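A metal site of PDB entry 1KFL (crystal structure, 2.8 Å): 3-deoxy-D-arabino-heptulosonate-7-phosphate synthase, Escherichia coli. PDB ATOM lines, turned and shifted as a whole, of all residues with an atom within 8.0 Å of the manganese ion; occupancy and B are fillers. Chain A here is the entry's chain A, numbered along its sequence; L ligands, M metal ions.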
ATOM      1  N   GLY A  59     -26.741 -30.873   3.320  1.00  0.00           N
ATOM      2  CA  GLY A  59     -26.134 -30.586   2.033  1.00  0.00           C
ATOM      3  C   GLY A  59     -24.611 -30.489   2.125  1.00  0.00           C
ATOM      4  O   GLY A  59     -24.029 -30.575   3.201  1.00  0.00           O
ATOM      5  N   PRO A  60     -23.933 -30.289   0.985  1.00  0.00           N
ATOM      6  CA  PRO A  60     -22.479 -30.194   0.966  1.00  0.00           C
ATOM      7  C   PRO A  60     -21.927 -29.231   2.004  1.00  0.00           C
ATOM      8  O   PRO A  60     -22.577 -28.266   2.388  1.00  0.00           O
ATOM      9  CB  PRO A  60     -22.185 -29.711  -0.443  1.00  0.00           C
ATOM     10  CG  PRO A  60     -23.292 -30.351  -1.227  1.00  0.00           C
ATOM     11  CD  PRO A  60     -24.476 -30.088  -0.359  1.00  0.00           C
ATOM     12  N   CYS A  61     -20.697 -29.508   2.445  1.00  0.00           N
ATOM     13  CA  CYS A  61     -20.005 -28.676   3.420  1.00  0.00           C
ATOM     14  C   CYS A  61     -19.888 -27.277   2.817  1.00  0.00           C
ATOM     15  O   CYS A  61     -20.131 -26.275   3.483  1.00  0.00           O
ATOM     16  CB  CYS A  61     -18.619 -29.256   3.690  1.00  0.00           C
ATOM     17  SG  CYS A  61     -17.494 -28.203   4.625  1.00  0.00           S
ATOM     18  N   SER A  62     -19.505 -27.261   1.551  1.00  0.00           N
ATOM     19  CA  SER A  62     -19.340 -26.035   0.780  1.00  0.00           C
ATOM     20  C   SER A  62     -19.661 -26.406  -0.678  1.00  0.00           C
ATOM     21  O   SER A  62     -19.574 -27.573  -1.064  1.00  0.00           O
ATOM     22  CB  SER A  62     -17.898 -25.528   0.872  1.00  0.00           C
ATOM     23  OG  SER A  62     -16.992 -26.427   0.261  1.00  0.00           O
ATOM     24  N   ARG A  92     -28.375 -27.257   2.382  1.00  0.00           N
ATOM     25  CA  ARG A  92     -27.282 -26.452   2.925  1.00  0.00           C
ATOM     26  C   ARG A  92     -26.460 -25.922   1.758  1.00  0.00           C
ATOM     27  O   ARG A  92     -25.668 -26.641   1.140  1.00  0.00           O
ATOM     28  CB  ARG A  92     -26.422 -27.320   3.851  1.00  0.00           C
ATOM     29  CG  ARG A  92     -25.187 -26.644   4.453  1.00  0.00           C
ATOM     30  CD  ARG A  92     -24.180 -27.691   4.939  1.00  0.00           C
ATOM     31  NE  ARG A  92     -22.828 -27.152   5.146  1.00  0.00           N
ATOM     32  CZ  ARG A  92     -22.405 -26.627   6.302  1.00  0.00           C
ATOM     33  NH1 ARG A  92     -23.221 -26.579   7.351  1.00  0.00           N
ATOM     34  NH2 ARG A  92     -21.167 -26.170   6.422  1.00  0.00           N
ATOM     35  N   TYR A  94     -23.741 -23.520   1.313  1.00  0.00           N
ATOM     36  CA  TYR A  94     -22.673 -22.655   1.872  1.00  0.00           C
ATOM     37  C   TYR A  94     -21.573 -22.522   0.833  1.00  0.00           C
ATOM     38  O   TYR A  94     -21.181 -23.513   0.218  1.00  0.00           O
ATOM     39  CB  TYR A  94     -22.055 -23.288   3.121  1.00  0.00           C
ATOM     40  CG  TYR A  94     -22.903 -23.246   4.380  1.00  0.00           C
ATOM     41  CD1 TYR A  94     -24.302 -23.333   4.321  1.00  0.00           C
ATOM     42  CD2 TYR A  94     -22.305 -23.189   5.628  1.00  0.00           C
ATOM     43  CE1 TYR A  94     -25.071 -23.362   5.487  1.00  0.00           C
ATOM     44  CE2 TYR A  94     -23.043 -23.229   6.783  1.00  0.00           C
ATOM     45  CZ  TYR A  94     -24.434 -23.315   6.719  1.00  0.00           C
ATOM     46  OH  TYR A  94     -25.169 -23.405   7.897  1.00  0.00           O
ATOM     47  N   GLU A  96     -18.421 -20.959   1.392  1.00  0.00           N
ATOM     48  CA  GLU A  96     -17.083 -20.874   1.906  1.00  0.00           C
ATOM     49  C   GLU A  96     -16.984 -21.325   3.360  1.00  0.00           C
ATOM     50  O   GLU A  96     -17.933 -21.173   4.144  1.00  0.00           O
ATOM     51  CB  GLU A  96     -16.580 -19.434   1.776  1.00  0.00           C
ATOM     52  CG  GLU A  96     -16.030 -18.856   3.085  1.00  0.00           C
ATOM     53  CD  GLU A  96     -15.436 -17.477   2.926  1.00  0.00           C
ATOM     54  OE1 GLU A  96     -16.188 -16.569   2.466  1.00  0.00           O
ATOM     55  OE2 GLU A  96     -14.251 -17.286   3.265  1.00  0.00           O
ATOM     56  N   LYS A  97     -15.839 -21.884   3.708  1.00  0.00           N
ATOM     57  CA  LYS A  97     -15.589 -22.316   5.063  1.00  0.00           C
ATOM     58  C   LYS A  97     -14.447 -21.461   5.605  1.00  0.00           C
ATOM     59  O   LYS A  97     -13.388 -21.349   4.982  1.00  0.00           O
ATOM     60  CB  LYS A  97     -15.186 -23.794   5.109  1.00  0.00           C
ATOM     61  CG  LYS A  97     -14.539 -24.165   6.430  1.00  0.00           C
ATOM     62  CD  LYS A  97     -14.820 -25.599   6.844  1.00  0.00           C
ATOM     63  CE  LYS A  97     -14.272 -25.819   8.247  1.00  0.00           C
ATOM     64  NZ  LYS A  97     -14.543 -27.180   8.776  1.00  0.00           N
ATOM     65  N   PRO A  98     -14.668 -20.819   6.761  1.00  0.00           N
ATOM     66  CA  PRO A  98     -13.643 -19.963   7.377  1.00  0.00           C
ATOM     67  C   PRO A  98     -12.383 -20.762   7.683  1.00  0.00           C
ATOM     68  O   PRO A  98     -12.455 -21.841   8.258  1.00  0.00           O
ATOM     69  CB  PRO A  98     -14.345 -19.460   8.643  1.00  0.00           C
ATOM     70  CG  PRO A  98     -15.772 -19.364   8.190  1.00  0.00           C
ATOM     71  CD  PRO A  98     -15.953 -20.669   7.458  1.00  0.00           C
ATOM     72  N   GLU A 143     -24.976 -19.447   5.204  1.00  0.00           N
ATOM     73  CA  GLU A 143     -24.324 -18.861   6.363  1.00  0.00           C
ATOM     74  C   GLU A 143     -23.995 -17.438   5.963  1.00  0.00           C
ATOM     75  O   GLU A 143     -23.955 -17.131   4.783  1.00  0.00           O
ATOM     76  CB  GLU A 143     -23.044 -19.650   6.678  1.00  0.00           C
ATOM     77  CG  GLU A 143     -22.176 -19.075   7.778  1.00  0.00           C
ATOM     78  CD  GLU A 143     -21.031 -19.994   8.147  1.00  0.00           C
ATOM     79  OE1 GLU A 143     -20.352 -20.530   7.222  1.00  0.00           O
ATOM     80  OE2 GLU A 143     -20.798 -20.189   9.359  1.00  0.00           O
ATOM     81  N   LYS A 186     -24.377 -20.963  16.359  1.00  0.00           N
ATOM     82  CA  LYS A 186     -23.629 -22.153  16.766  1.00  0.00           C
ATOM     83  C   LYS A 186     -22.928 -21.944  18.083  1.00  0.00           C
ATOM     84  O   LYS A 186     -22.454 -20.857  18.355  1.00  0.00           O
ATOM     85  CB  LYS A 186     -22.600 -22.510  15.691  1.00  0.00           C
ATOM     86  CG  LYS A 186     -23.243 -23.048  14.424  1.00  0.00           C
ATOM     87  CD  LYS A 186     -22.244 -23.900  13.668  1.00  0.00           C
ATOM     88  CE  LYS A 186     -22.930 -24.988  12.857  1.00  0.00           C
ATOM     89  NZ  LYS A 186     -21.918 -26.004  12.406  1.00  0.00           N
ATOM     90  N   ASP A 265     -26.064 -30.415  15.157  1.00  0.00           N
ATOM     91  CA  ASP A 265     -25.229 -30.605  13.985  1.00  0.00           C
ATOM     92  C   ASP A 265     -24.545 -31.971  14.107  1.00  0.00           C
ATOM     93  O   ASP A 265     -23.688 -32.180  14.984  1.00  0.00           O
ATOM     94  CB  ASP A 265     -24.187 -29.463  13.898  1.00  0.00           C
ATOM     95  CG  ASP A 265     -23.317 -29.555  12.636  1.00  0.00           C
ATOM     96  OD1 ASP A 265     -23.655 -30.354  11.735  1.00  0.00           O
ATOM     97  OD2 ASP A 265     -22.305 -28.813  12.531  1.00  0.00           O
ATOM     98  N   SER A 267     -22.478 -33.102  12.159  1.00  0.00           N
ATOM     99  CA  SER A 267     -21.106 -32.998  11.641  1.00  0.00           C
ATOM    100  C   SER A 267     -20.146 -32.197  12.492  1.00  0.00           C
ATOM    101  O   SER A 267     -20.415 -31.945  13.656  1.00  0.00           O
ATOM    102  CB  SER A 267     -21.138 -32.456  10.210  1.00  0.00           C
ATOM    103  OG  SER A 267     -19.876 -32.584   9.579  1.00  0.00           O
ATOM    104  N   HIS A 268     -19.003 -31.834  11.914  1.00  0.00           N
ATOM    105  CA  HIS A 268     -17.985 -31.066  12.624  1.00  0.00           C
ATOM    106  C   HIS A 268     -17.574 -31.678  13.964  1.00  0.00           C
ATOM    107  O   HIS A 268     -17.326 -32.886  14.032  1.00  0.00           O
ATOM    108  CB  HIS A 268     -18.453 -29.615  12.776  1.00  0.00           C
ATOM    109  CG  HIS A 268     -18.862 -29.002  11.472  1.00  0.00           C
ATOM    110  ND1 HIS A 268     -20.156 -29.056  11.000  1.00  0.00           N
ATOM    111  CD2 HIS A 268     -18.115 -28.469  10.473  1.00  0.00           C
ATOM    112  CE1 HIS A 268     -20.179 -28.611   9.750  1.00  0.00           C
ATOM    113  NE2 HIS A 268     -18.957 -28.253   9.412  1.00  0.00           N
ATOM    114  N   MET A 300     -28.579 -30.888  11.455  1.00  0.00           N
ATOM    115  CA  MET A 300     -27.788 -30.448  10.314  1.00  0.00           C
ATOM    116  C   MET A 300     -26.813 -31.562   9.917  1.00  0.00           C
ATOM    117  O   MET A 300     -26.115 -32.123  10.770  1.00  0.00           O
ATOM    118  CB  MET A 300     -26.992 -29.187  10.667  1.00  0.00           C
ATOM    119  CG  MET A 300     -26.255 -28.558   9.500  1.00  0.00           C
ATOM    120  SD  MET A 300     -25.430 -26.922  10.121  1.00  0.00           S
ATOM    121  CE  MET A 300     -23.601 -27.473  10.250  1.00  0.00           C
ATOM    122  N   GLU A 302     -23.781 -32.750   6.971  1.00  0.00           N
ATOM    123  CA  GLU A 302     -22.931 -32.470   5.827  1.00  0.00           C
ATOM    124  C   GLU A 302     -22.968 -33.708   4.937  1.00  0.00           C
ATOM    125  O   GLU A 302     -22.431 -34.738   5.310  1.00  0.00           O
ATOM    126  CB  GLU A 302     -21.491 -32.155   6.274  1.00  0.00           C
ATOM    127  CG  GLU A 302     -21.388 -30.830   7.001  1.00  0.00           C
ATOM    128  CD  GLU A 302     -19.955 -30.303   7.099  1.00  0.00           C
ATOM    129  OE1 GLU A 302     -19.119 -30.967   7.753  1.00  0.00           O
ATOM    130  OE2 GLU A 302     -19.668 -29.213   6.527  1.00  0.00           O
ATOM    131  N   SER A 323     -17.035 -33.261  -1.866  1.00  0.00           N
ATOM    132  CA  SER A 323     -16.568 -32.094  -1.118  1.00  0.00           C
ATOM    133  C   SER A 323     -15.084 -31.823  -1.300  1.00  0.00           C
ATOM    134  O   SER A 323     -14.315 -32.744  -1.524  1.00  0.00           O
ATOM    135  CB  SER A 323     -16.877 -32.286   0.370  1.00  0.00           C
ATOM    136  OG  SER A 323     -16.282 -31.249   1.126  1.00  0.00           O
ATOM    137  N   THR A 325     -13.819 -29.573   0.935  1.00  0.00           N
ATOM    138  CA  THR A 325     -13.607 -29.006   2.258  1.00  0.00           C
ATOM    139  C   THR A 325     -13.846 -30.178   3.232  1.00  0.00           C
ATOM    140  O   THR A 325     -13.239 -31.228   3.093  1.00  0.00           O
ATOM    141  CB  THR A 325     -14.572 -27.813   2.583  1.00  0.00           C
ATOM    142  OG1 THR A 325     -15.879 -28.068   2.062  1.00  0.00           O
ATOM    143  CG2 THR A 325     -14.037 -26.532   2.010  1.00  0.00           C
ATOM    144  N   ASP A 326     -14.750 -30.012   4.194  1.00  0.00           N
ATOM    145  CA  ASP A 326     -15.013 -31.094   5.133  1.00  0.00           C
ATOM    146  C   ASP A 326     -15.571 -32.321   4.429  1.00  0.00           C
ATOM    147  O   ASP A 326     -16.240 -32.203   3.404  1.00  0.00           O
ATOM    148  CB  ASP A 326     -15.987 -30.636   6.215  1.00  0.00           C
ATOM    149  CG  ASP A 326     -15.429 -29.517   7.071  1.00  0.00           C
ATOM    150  OD1 ASP A 326     -14.190 -29.372   7.098  1.00  0.00           O
ATOM    151  OD2 ASP A 326     -16.227 -28.807   7.732  1.00  0.00           O
ATOM    152  N   ALA A 327     -15.283 -33.499   4.989  1.00  0.00           N
ATOM    153  CA  ALA A 327     -15.756 -34.762   4.434  1.00  0.00           C
ATOM    154  C   ALA A 327     -17.257 -34.892   4.676  1.00  0.00           C
ATOM    155  O   ALA A 327     -17.743 -34.513   5.747  1.00  0.00           O
ATOM    156  CB  ALA A 327     -15.034 -35.896   5.108  1.00  0.00           C
ATOM    157  N   CYS A 328     -17.988 -35.434   3.711  1.00  0.00           N
ATOM    158  CA  CYS A 328     -19.430 -35.587   3.847  1.00  0.00           C
ATOM    159  C   CYS A 328     -19.849 -37.033   3.605  1.00  0.00           C
ATOM    160  O   CYS A 328     -19.165 -37.765   2.892  1.00  0.00           O
ATOM    161  CB  CYS A 328     -20.178 -34.699   2.838  1.00  0.00           C
ATOM    162  SG  CYS A 328     -19.685 -32.978   2.807  1.00  0.00           S
HETATM  163  C1  LIG L   1     -18.315 -25.483  12.817  1.00  0.00           C
HETATM  164  O1  LIG L   1     -17.360 -25.074  13.582  1.00  0.00           O
HETATM  165  O2  LIG L   1     -19.040 -26.380  13.111  1.00  0.00           O
HETATM  166  C2  LIG L   1     -18.442 -24.739  11.489  1.00  0.00           C
HETATM  167  C3  LIG L   1     -17.705 -23.696  11.008  1.00  0.00           C
HETATM  168  O3  LIG L   1     -19.484 -25.229  10.691  1.00  0.00           O
HETATM  169  P1  LIG L   1     -20.349 -24.443   9.608  1.00  0.00           P
HETATM  170  O4  LIG L   1     -21.604 -25.314   9.336  1.00  0.00           O
HETATM  171  O5  LIG L   1     -19.461 -24.304   8.402  1.00  0.00           O
HETATM  172  O6  LIG L   1     -20.773 -23.171  10.278  1.00  0.00           O
HETATM  173 MN    MN M   1     -18.070 -28.034   7.210  1.00  0.00          MN
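A ring nitrogen (NE2) of His 268 sits close to an oxygen (O3) of the ligand, 3.3 Å away. An oxygen (O2) of the ligand lies within salt-bridge range of the side-chain amino group (NZ) of Lys 186, 3.0 Å away. The guanidinium group of Arg 92 is in salt-bridge range of an oxygen (O4) of the ligand, at 2.9 Å.
The side-chain sulfur (SG) of Cys 328 lies within hydrogen-bond range of the backbone NH (N) of Cys 61 (3.6 Å). The guanidinium group (NH2) of Arg 92 lies within hydrogen-bond range of the backbone carbonyl oxygen (O) of Cys 61 (3.1 Å). OE1 of Glu 302 lies within hydrogen-bond range of OG of Ser 267. The side-chain carboxylate (OD1) of Asp 326 is in salt-bridge range of the side-chain amino group (NZ) of Lys 97. ND1 of His 268 sits at hydrogen-bond distance from OD2 of Asp 265, 2.6 Å away. OE2 of Glu 302 sits close to NH2 of Arg 92. O of Asp 326 lies within hydrogen-bond range of OG of Ser 323 (2.5 Å). The backbone carbonyl oxygen (O) of Asp 326 lies within hydrogen-bond range of the side-chain sulfur (SG) of Cys 328 (3.6 Å).
NH2 of Arg 92 touches the manganese ion, at 3.7 Å. NZ of Lys 97 touches the manganese ion, at 3.95 Å. Six residues have an atom within 4 Å of the manganese ion: Cys 61, Arg 92, Lys 97, His 268, Glu 302 and Asp 326. The nearest printed residue that does not touch the manganese ion is Ser 267 (5.4 Å).
The manganese ion is bound by the side-chain carboxylate (OD2) of Asp 326. The manganese ion is bound by OE2 of Glu 302, 2.1 Å away. A ring nitrogen (NE2) of His 268 is bound to the manganese ion. The side-chain sulfur (SG) of Cys 61 binds the manganese ion (2.7 Å).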
